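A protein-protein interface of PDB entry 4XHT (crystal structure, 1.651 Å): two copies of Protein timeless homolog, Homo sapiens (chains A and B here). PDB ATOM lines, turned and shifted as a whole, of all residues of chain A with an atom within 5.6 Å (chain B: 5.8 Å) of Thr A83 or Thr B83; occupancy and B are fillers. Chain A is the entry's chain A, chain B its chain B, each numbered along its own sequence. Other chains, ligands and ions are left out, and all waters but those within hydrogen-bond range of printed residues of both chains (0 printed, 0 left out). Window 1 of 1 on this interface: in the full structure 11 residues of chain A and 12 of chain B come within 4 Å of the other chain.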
ATOM      1  N   PRO A  51       6.347 -13.597 -14.099  1.00  0.00           N
ATOM      2  CA  PRO A  51       7.191 -14.789 -14.260  1.00  0.00           C
ATOM      3  C   PRO A  51       8.500 -14.605 -13.489  1.00  0.00           C
ATOM      4  O   PRO A  51       9.297 -13.722 -13.798  1.00  0.00           O
ATOM      5  CB  PRO A  51       7.410 -14.856 -15.773  1.00  0.00           C
ATOM      6  CG  PRO A  51       7.385 -13.374 -16.207  1.00  0.00           C
ATOM      7  CD  PRO A  51       6.335 -12.741 -15.306  1.00  0.00           C
ATOM      8  N   GLU A  57       9.194 -17.230 -17.700  1.00  0.00           N
ATOM      9  CA  GLU A  57       9.376 -16.178 -18.687  1.00  0.00           C
ATOM     10  C   GLU A  57       9.170 -16.726 -20.093  1.00  0.00           C
ATOM     11  O   GLU A  57       8.457 -16.141 -20.905  1.00  0.00           O
ATOM     12  CB  GLU A  57      10.774 -15.577 -18.578  1.00  0.00           C
ATOM     13  CG  GLU A  57      10.901 -14.366 -17.724  1.00  0.00           C
ATOM     14  CD  GLU A  57      12.316 -13.814 -17.812  1.00  0.00           C
ATOM     15  OE1 GLU A  57      13.198 -14.245 -17.015  1.00  0.00           O
ATOM     16  OE2 GLU A  57      12.545 -13.010 -18.742  1.00  0.00           O
ATOM     17  N   MET A  60       5.568 -17.269 -20.828  1.00  0.00           N
ATOM     18  CA  MET A  60       4.835 -16.026 -21.067  1.00  0.00           C
ATOM     19  C   MET A  60       5.132 -15.424 -22.444  1.00  0.00           C
ATOM     20  O   MET A  60       4.365 -14.582 -22.933  1.00  0.00           O
ATOM     21  CB  MET A  60       5.141 -14.986 -19.980  1.00  0.00           C
ATOM     22  CG  MET A  60       4.550 -15.331 -18.609  1.00  0.00           C
ATOM     23  SD  MET A  60       2.757 -15.634 -18.699  1.00  0.00           S
ATOM     24  CE  MET A  60       2.192 -14.104 -19.438  1.00  0.00           C
ATOM     25  N   GLU A  61       6.238 -15.835 -23.065  1.00  0.00           N
ATOM     26  CA  GLU A  61       6.593 -15.315 -24.386  1.00  0.00           C
ATOM     27  C   GLU A  61       6.219 -16.291 -25.496  1.00  0.00           C
ATOM     28  O   GLU A  61       6.466 -16.023 -26.676  1.00  0.00           O
ATOM     29  CB  GLU A  61       8.088 -14.986 -24.447  1.00  0.00           C
ATOM     30  CG  GLU A  61       8.526 -13.946 -23.421  1.00  0.00           C
ATOM     31  CD  GLU A  61       7.786 -12.617 -23.536  1.00  0.00           C
ATOM     32  OE1 GLU A  61       7.405 -12.226 -24.662  1.00  0.00           O
ATOM     33  OE2 GLU A  61       7.552 -11.980 -22.486  1.00  0.00           O
ATOM     34  N   PRO A  77      -0.939  -7.145 -21.252  1.00  0.00           N
ATOM     35  CA  PRO A  77      -0.524  -5.881 -20.638  1.00  0.00           C
ATOM     36  C   PRO A  77      -0.875  -4.687 -21.501  1.00  0.00           C
ATOM     37  O   PRO A  77      -0.974  -4.809 -22.714  1.00  0.00           O
ATOM     38  CB  PRO A  77       0.997  -6.022 -20.506  1.00  0.00           C
ATOM     39  CG  PRO A  77       1.389  -7.063 -21.480  1.00  0.00           C
ATOM     40  CD  PRO A  77       0.210  -7.998 -21.600  1.00  0.00           C
ATOM     41  N   ALA A  78      -1.124  -3.561 -20.857  1.00  0.00           N
ATOM     42  CA  ALA A  78      -1.284  -2.301 -21.588  1.00  0.00           C
ATOM     43  C   ALA A  78       0.068  -1.889 -22.168  1.00  0.00           C
ATOM     44  O   ALA A  78       1.013  -1.607 -21.426  1.00  0.00           O
ATOM     45  CB  ALA A  78      -1.834  -1.231 -20.678  1.00  0.00           C
ATOM     46  N   GLN A  81       2.770   0.753 -20.818  1.00  0.00           N
ATOM     47  CA  GLN A  81       2.423   1.015 -19.423  1.00  0.00           C
ATOM     48  C   GLN A  81       2.728  -0.167 -18.510  1.00  0.00           C
ATOM     49  O   GLN A  81       3.188   0.016 -17.386  1.00  0.00           O
ATOM     50  CB  GLN A  81       0.935   1.356 -19.298  1.00  0.00           C
ATOM     51  CG  GLN A  81       0.522   2.601 -20.071  1.00  0.00           C
ATOM     52  CD  GLN A  81       1.185   3.860 -19.532  1.00  0.00           C
ATOM     53  OE1 GLN A  81       1.328   4.020 -18.320  1.00  0.00           O
ATOM     54  NE2 GLN A  81       1.593   4.759 -20.432  1.00  0.00           N
ATOM     55  N   GLU A  82       2.434  -1.366 -18.998  1.00  0.00           N
ATOM     56  CA  GLU A  82       2.587  -2.592 -18.216  1.00  0.00           C
ATOM     57  C   GLU A  82       3.524  -3.585 -18.865  1.00  0.00           C
ATOM     58  O   GLU A  82       3.603  -3.664 -20.088  1.00  0.00           O
ATOM     59  CB  GLU A  82       1.228  -3.260 -18.014  1.00  0.00           C
ATOM     60  CG  GLU A  82       0.278  -2.476 -17.128  1.00  0.00           C
ATOM     61  CD  GLU A  82      -1.121  -3.058 -17.140  1.00  0.00           C
ATOM     62  OE1 GLU A  82      -1.459  -3.773 -18.103  1.00  0.00           O
ATOM     63  OE2 GLU A  82      -1.864  -2.826 -16.171  1.00  0.00           O
ATOM     64  N   THR A  83       4.194  -4.373 -18.023  1.00  0.00           N
ATOM     65  CA  THR A  83       4.979  -5.515 -18.466  1.00  0.00           C
ATOM     66  C   THR A  83       4.118  -6.784 -18.424  1.00  0.00           C
ATOM     67  O   THR A  83       4.209  -7.636 -19.305  1.00  0.00           O
ATOM     68  CB  THR A  83       6.222  -5.731 -17.567  1.00  0.00           C
ATOM     69  OG1 THR A  83       7.015  -4.528 -17.534  1.00  0.00           O
ATOM     70  CG2 THR A  83       7.076  -6.878 -18.085  1.00  0.00           C
ATOM     71  N   PHE A  84       3.292  -6.903 -17.393  1.00  0.00           N
ATOM     72  CA  PHE A  84       2.640  -8.196 -17.103  1.00  0.00           C
ATOM     73  C   PHE A  84       1.200  -8.310 -17.576  1.00  0.00           C
ATOM     74  O   PHE A  84       0.437  -7.341 -17.553  1.00  0.00           O
ATOM     75  CB  PHE A  84       2.668  -8.475 -15.591  1.00  0.00           C
ATOM     76  CG  PHE A  84       4.045  -8.331 -14.988  1.00  0.00           C
ATOM     77  CD1 PHE A  84       5.098  -9.111 -15.446  1.00  0.00           C
ATOM     78  CD2 PHE A  84       4.291  -7.386 -13.991  1.00  0.00           C
ATOM     79  CE1 PHE A  84       6.388  -8.962 -14.918  1.00  0.00           C
ATOM     80  CE2 PHE A  84       5.582  -7.226 -13.454  1.00  0.00           C
ATOM     81  CZ  PHE A  84       6.631  -8.020 -13.923  1.00  0.00           C
ATOM     82  N   TRP A  85       0.839  -9.521 -17.989  1.00  0.00           N
ATOM     83  CA  TRP A  85      -0.562  -9.886 -18.170  1.00  0.00           C
ATOM     84  C   TRP A  85      -1.277  -9.784 -16.819  1.00  0.00           C
ATOM     85  O   TRP A  85      -0.642  -9.922 -15.761  1.00  0.00           O
ATOM     86  CB  TRP A  85      -0.679 -11.311 -18.718  1.00  0.00           C
ATOM     87  CG  TRP A  85      -0.204 -11.469 -20.129  1.00  0.00           C
ATOM     88  CD1 TRP A  85       1.056 -11.248 -20.605  1.00  0.00           C
ATOM     89  CD2 TRP A  85      -0.988 -11.906 -21.250  1.00  0.00           C
ATOM     90  NE1 TRP A  85       1.105 -11.506 -21.963  1.00  0.00           N
ATOM     91  CE2 TRP A  85      -0.130 -11.920 -22.373  1.00  0.00           C
ATOM     92  CE3 TRP A  85      -2.322 -12.291 -21.407  1.00  0.00           C
ATOM     93  CZ2 TRP A  85      -0.579 -12.293 -23.645  1.00  0.00           C
ATOM     94  CZ3 TRP A  85      -2.763 -12.661 -22.670  1.00  0.00           C
ATOM     95  CH2 TRP A  85      -1.890 -12.660 -23.773  1.00  0.00           C
ATOM     96  N   ARG A  86      -2.585  -9.540 -16.850  1.00  0.00           N
ATOM     97  CA  ARG A  86      -3.374  -9.402 -15.625  1.00  0.00           C
ATOM     98  C   ARG A  86      -4.556 -10.372 -15.569  1.00  0.00           C
ATOM     99  O   ARG A  86      -5.236 -10.576 -16.567  1.00  0.00           O
ATOM    100  CB  ARG A  86      -3.940  -7.990 -15.489  1.00  0.00           C
ATOM    101  CG  ARG A  86      -3.260  -7.086 -14.479  1.00  0.00           C
ATOM    102  CD  ARG A  86      -1.912  -6.616 -14.991  1.00  0.00           C
ATOM    103  NE  ARG A  86      -1.268  -5.748 -14.007  1.00  0.00           N
ATOM    104  CZ  ARG A  86      -0.046  -5.246 -14.147  1.00  0.00           C
ATOM    105  NH1 ARG A  86       0.671  -5.527 -15.229  1.00  0.00           N
ATOM    106  NH2 ARG A  86       0.466  -4.486 -13.187  1.00  0.00           N
ATOM    107  N   PRO B  51      10.780  -5.758 -12.459  1.00  0.00           N
ATOM    108  CA  PRO B  51       9.912  -4.780 -11.805  1.00  0.00           C
ATOM    109  C   PRO B  51       8.750  -5.449 -11.096  1.00  0.00           C
ATOM    110  O   PRO B  51       8.046  -6.220 -11.731  1.00  0.00           O
ATOM    111  CB  PRO B  51       9.419  -3.917 -12.972  1.00  0.00           C
ATOM    112  CG  PRO B  51       9.440  -4.836 -14.158  1.00  0.00           C
ATOM    113  CD  PRO B  51      10.651  -5.727 -13.928  1.00  0.00           C
ATOM    114  N   GLU B  57       7.174  -1.081 -13.279  1.00  0.00           N
ATOM    115  CA  GLU B  57       6.700  -1.535 -14.590  1.00  0.00           C
ATOM    116  C   GLU B  57       6.556  -0.383 -15.573  1.00  0.00           C
ATOM    117  O   GLU B  57       7.005  -0.461 -16.716  1.00  0.00           O
ATOM    118  CB  GLU B  57       5.334  -2.197 -14.476  1.00  0.00           C
ATOM    119  CG  GLU B  57       5.328  -3.628 -14.309  1.00  0.00           C
ATOM    120  CD  GLU B  57       3.888  -4.117 -14.340  1.00  0.00           C
ATOM    121  OE1 GLU B  57       3.245  -4.082 -13.271  1.00  0.00           O
ATOM    122  OE2 GLU B  57       3.414  -4.507 -15.422  1.00  0.00           O
ATOM    123  N   MET B  60       9.839   0.736 -16.787  1.00  0.00           N
ATOM    124  CA  MET B  60      10.461  -0.210 -17.706  1.00  0.00           C
ATOM    125  C   MET B  60       9.824  -0.187 -19.092  1.00  0.00           C
ATOM    126  O   MET B  60      10.436  -0.649 -20.056  1.00  0.00           O
ATOM    127  CB  MET B  60      10.410  -1.644 -17.141  1.00  0.00           C
ATOM    128  CG  MET B  60      11.331  -1.872 -15.925  1.00  0.00           C
ATOM    129  SD  MET B  60      13.068  -1.465 -16.253  1.00  0.00           S
ATOM    130  CE  MET B  60      13.333  -2.527 -17.663  1.00  0.00           C
ATOM    131  N   GLU B  61       8.608   0.343 -19.196  1.00  0.00           N
ATOM    132  CA  GLU B  61       7.917   0.409 -20.485  1.00  0.00           C
ATOM    133  C   GLU B  61       7.986   1.805 -21.118  1.00  0.00           C
ATOM    134  O   GLU B  61       7.436   2.037 -22.205  1.00  0.00           O
ATOM    135  CB  GLU B  61       6.452  -0.016 -20.331  1.00  0.00           C
ATOM    136  CG  GLU B  61       6.259  -1.439 -19.816  1.00  0.00           C
ATOM    137  CD  GLU B  61       6.918  -2.484 -20.704  1.00  0.00           C
ATOM    138  OE1 GLU B  61       7.028  -2.243 -21.934  1.00  0.00           O
ATOM    139  OE2 GLU B  61       7.294  -3.554 -20.176  1.00  0.00           O
ATOM    140  N   PRO B  77      15.190  -7.483 -23.486  1.00  0.00           N
ATOM    141  CA  PRO B  77      14.968  -8.928 -23.471  1.00  0.00           C
ATOM    142  C   PRO B  77      15.072  -9.524 -24.863  1.00  0.00           C
ATOM    143  O   PRO B  77      14.757  -8.848 -25.846  1.00  0.00           O
ATOM    144  CB  PRO B  77      13.544  -9.067 -22.925  1.00  0.00           C
ATOM    145  CG  PRO B  77      12.901  -7.735 -23.156  1.00  0.00           C
ATOM    146  CD  PRO B  77      13.997  -6.722 -23.073  1.00  0.00           C
ATOM    147  N   ALA B  78      15.525 -10.772 -24.933  1.00  0.00           N
ATOM    148  CA  ALA B  78      15.546 -11.524 -26.180  1.00  0.00           C
ATOM    149  C   ALA B  78      14.121 -11.819 -26.617  1.00  0.00           C
ATOM    150  O   ALA B  78      13.399 -12.526 -25.924  1.00  0.00           O
ATOM    151  CB  ALA B  78      16.333 -12.806 -26.018  1.00  0.00           C
ATOM    152  N   GLN B  81      11.671 -15.024 -26.123  1.00  0.00           N
ATOM    153  CA  GLN B  81      12.304 -15.908 -25.150  1.00  0.00           C
ATOM    154  C   GLN B  81      12.292 -15.333 -23.736  1.00  0.00           C
ATOM    155  O   GLN B  81      12.088 -16.055 -22.759  1.00  0.00           O
ATOM    156  CB  GLN B  81      13.743 -16.201 -25.576  1.00  0.00           C
ATOM    157  CG  GLN B  81      14.461 -17.216 -24.705  1.00  0.00           C
ATOM    158  CD  GLN B  81      14.000 -18.642 -24.978  1.00  0.00           C
ATOM    159  OE1 GLN B  81      13.278 -18.901 -25.943  1.00  0.00           O
ATOM    160  NE2 GLN B  81      14.419 -19.574 -24.128  1.00  0.00           N
ATOM    161  N   GLU B  82      12.525 -14.029 -23.634  1.00  0.00           N
ATOM    162  CA  GLU B  82      12.613 -13.361 -22.344  1.00  0.00           C
ATOM    163  C   GLU B  82      11.562 -12.276 -22.184  1.00  0.00           C
ATOM    164  O   GLU B  82      11.143 -11.656 -23.157  1.00  0.00           O
ATOM    165  CB  GLU B  82      13.992 -12.726 -22.165  1.00  0.00           C
ATOM    166  CG  GLU B  82      15.128 -13.722 -22.078  1.00  0.00           C
ATOM    167  CD  GLU B  82      16.478 -13.033 -22.127  1.00  0.00           C
ATOM    168  OE1 GLU B  82      16.538 -11.882 -22.613  1.00  0.00           O
ATOM    169  OE2 GLU B  82      17.473 -13.642 -21.677  1.00  0.00           O
ATOM    170  N   THR B  83      11.159 -12.042 -20.940  1.00  0.00           N
ATOM    171  CA  THR B  83      10.306 -10.910 -20.592  1.00  0.00           C
ATOM    172  C   THR B  83      11.128  -9.703 -20.157  1.00  0.00           C
ATOM    173  O   THR B  83      10.825  -8.562 -20.523  1.00  0.00           O
ATOM    174  CB  THR B  83       9.349 -11.266 -19.450  1.00  0.00           C
ATOM    175  OG1 THR B  83       8.566 -12.401 -19.829  1.00  0.00           O
ATOM    176  CG2 THR B  83       8.432 -10.093 -19.144  1.00  0.00           C
ATOM    177  N   PHE B  84      12.186  -9.969 -19.397  1.00  0.00           N
ATOM    178  CA  PHE B  84      12.911  -8.902 -18.704  1.00  0.00           C
ATOM    179  C   PHE B  84      14.183  -8.428 -19.394  1.00  0.00           C
ATOM    180  O   PHE B  84      14.894  -9.204 -20.045  1.00  0.00           O
ATOM    181  CB  PHE B  84      13.270  -9.347 -17.278  1.00  0.00           C
ATOM    182  CG  PHE B  84      12.083  -9.767 -16.462  1.00  0.00           C
ATOM    183  CD1 PHE B  84      11.081  -8.857 -16.187  1.00  0.00           C
ATOM    184  CD2 PHE B  84      11.981 -11.056 -15.959  1.00  0.00           C
ATOM    185  CE1 PHE B  84       9.967  -9.228 -15.441  1.00  0.00           C
ATOM    186  CE2 PHE B  84      10.872 -11.443 -15.207  1.00  0.00           C
ATOM    187  CZ  PHE B  84       9.868 -10.519 -14.944  1.00  0.00           C
ATOM    188  N   TRP B  85      14.450  -7.137 -19.231  1.00  0.00           N
ATOM    189  CA  TRP B  85      15.758  -6.583 -19.554  1.00  0.00           C
ATOM    190  C   TRP B  85      16.806  -7.284 -18.691  1.00  0.00           C
ATOM    191  O   TRP B  85      16.496  -7.766 -17.600  1.00  0.00           O
ATOM    192  CB  TRP B  85      15.781  -5.067 -19.319  1.00  0.00           C
ATOM    193  CG  TRP B  85      14.994  -4.268 -20.308  1.00  0.00           C
ATOM    194  CD1 TRP B  85      13.650  -4.329 -20.539  1.00  0.00           C
ATOM    195  CD2 TRP B  85      15.513  -3.273 -21.206  1.00  0.00           C
ATOM    196  NE1 TRP B  85      13.299  -3.437 -21.534  1.00  0.00           N
ATOM    197  CE2 TRP B  85      14.426  -2.781 -21.957  1.00  0.00           C
ATOM    198  CE3 TRP B  85      16.795  -2.771 -21.457  1.00  0.00           C
ATOM    199  CZ2 TRP B  85      14.580  -1.799 -22.936  1.00  0.00           C
ATOM    200  CZ3 TRP B  85      16.945  -1.793 -22.425  1.00  0.00           C
ATOM    201  CH2 TRP B  85      15.844  -1.318 -23.150  1.00  0.00           C
ATOM    202  N   ARG B  86      18.041  -7.343 -19.185  1.00  0.00           N
ATOM    203  CA  ARG B  86      19.134  -8.005 -18.472  1.00  0.00           C
ATOM    204  C   ARG B  86      20.301  -7.054 -18.176  1.00  0.00           C
ATOM    205  O   ARG B  86      20.668  -6.240 -19.013  1.00  0.00           O
ATOM    206  CB  ARG B  86      19.665  -9.195 -19.286  1.00  0.00           C
ATOM    207  CG  ARG B  86      19.264 -10.555 -18.751  1.00  0.00           C
ATOM    208  CD  ARG B  86      17.794 -10.835 -18.967  1.00  0.00           C
ATOM    209  NE  ARG B  86      17.440 -12.126 -18.387  1.00  0.00           N
ATOM    210  CZ  ARG B  86      16.201 -12.608 -18.362  1.00  0.00           C
ATOM    211  NH1 ARG B  86      15.211 -11.907 -18.903  1.00  0.00           N
ATOM    212  NH2 ARG B  86      15.957 -13.787 -17.798  1.00  0.00           N
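The side-chain carboxylate (OE2) of Glu A57 is in hydrogen-bond range of the backbone NH (N) of Thr B83, 2.8 Å away.
N of Phe B84 is in hydrogen-bond range of OE2 of Glu A57, 3.1 Å away.
OE2 of Glu A57 lies within salt-bridge range of NH1 of Arg B86, at 2.9 Å.
The side-chain hydroxyl of Thr B83 lies within hydrogen-bond range of the side-chain carboxylate of Glu A61.
The side-chain carboxylate (OE2) of Glu B57 sits at hydrogen-bond distance from the backbone NH (N) of Thr A83.
OE2 of Glu B61 sits at hydrogen-bond distance from OG1 of Thr A83 (2.8 Å).
N of Phe A84 lies within hydrogen-bond range of OE2 of Glu B57.
The guanidinium group of Arg A86 lies within salt-bridge range of the side-chain carboxylate of Glu B57 (2.8 Å).
OE1 of Glu A82 sits at hydrogen-bond distance from N of Ala A78.
The side-chain carboxylate (OE2) of Glu A82 is in salt-bridge range of the guanidinium group (NE) of Arg A86, 3.7 Å away.
The guanidinium group (NH1) of Arg A86 lies within hydrogen-bond range of the backbone carbonyl oxygen (O) of Phe A84 (3.0 Å).
The side-chain carboxylate of Glu B82 is in hydrogen-bond range of the backbone NH of Ala B78, 2.8 Å away.
The side-chain carboxylate of Glu B82 is in salt-bridge range of the guanidinium group of Arg B86.
The backbone carbonyl oxygen (O) of Phe B84 is in hydrogen-bond range of the guanidinium group (NH1) of Arg B86.
Among the printed residues, pairs that only touch across the chains: Pro A51 with Phe B84, Phe A84 with Pro B51, Glu A82 with Glu B61, Glu A82 with Glu B57, Glu A61 with Glu B82, Glu A57 with Glu B82, Phe A84 with Phe B84, Thr A83 with Thr B83, Gln A81 with Glu B61, Gln A81 with Glu B57, Pro A51 with Thr B83 and Glu A61 with Gln B81.
Printed residues of chain B within 4 Å of Glu A61: Gln B81, Glu B82 and Thr B83.
Ala A78 touches none of the printed residues of chain B.
Of the printed residues of chain B, Thr A83 touches Glu B57, Glu B61 and Thr B83.
Pro B77 touches none of the printed residues of chain A.
Printed residues of chain A within 4 Å of Glu B82: Glu A57 and Glu A61.
Thr B83 touches just these residues of chain A: Pro A51, Glu A57, Glu A61 and Thr A83.
The nearest residue of chain B that does not touch Thr A83 is Pro B51 (4.2 Å).
Of the 12 printed residues of chain A, 8 touch a printed residue of chain B.
Hydrophobic or aromatic side chains of chain A within 4 Å of the printed part of chain B: Pro A51 and Phe A84.
Among the printed residues, 20 pairs touch across the chains.
Among the printed residues, Asp or Glu carboxylates within 4 Å of a Lys or Arg side-chain nitrogen of the other chain: Glu A57 with Arg B86 (2.9 Å) and Arg A86 with Glu B57 (2.8 Å).
Pro A51 touches Phe B84, and with the chains exchanged Phe A84 touches Pro B51.
Glu A57 touches Glu B82, and with the chains exchanged Glu A82 touches Glu B57.
Glu A61 touches Glu B82, and with the chains exchanged Glu A82 touches Glu B61.
Phe B84 touches its own counterpart, Phe A84.
12 positions are printed for both chains.
Of the 20 pairs that touch across the chains among the printed residues, 18 have their exchanged pair printed and touching as well.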
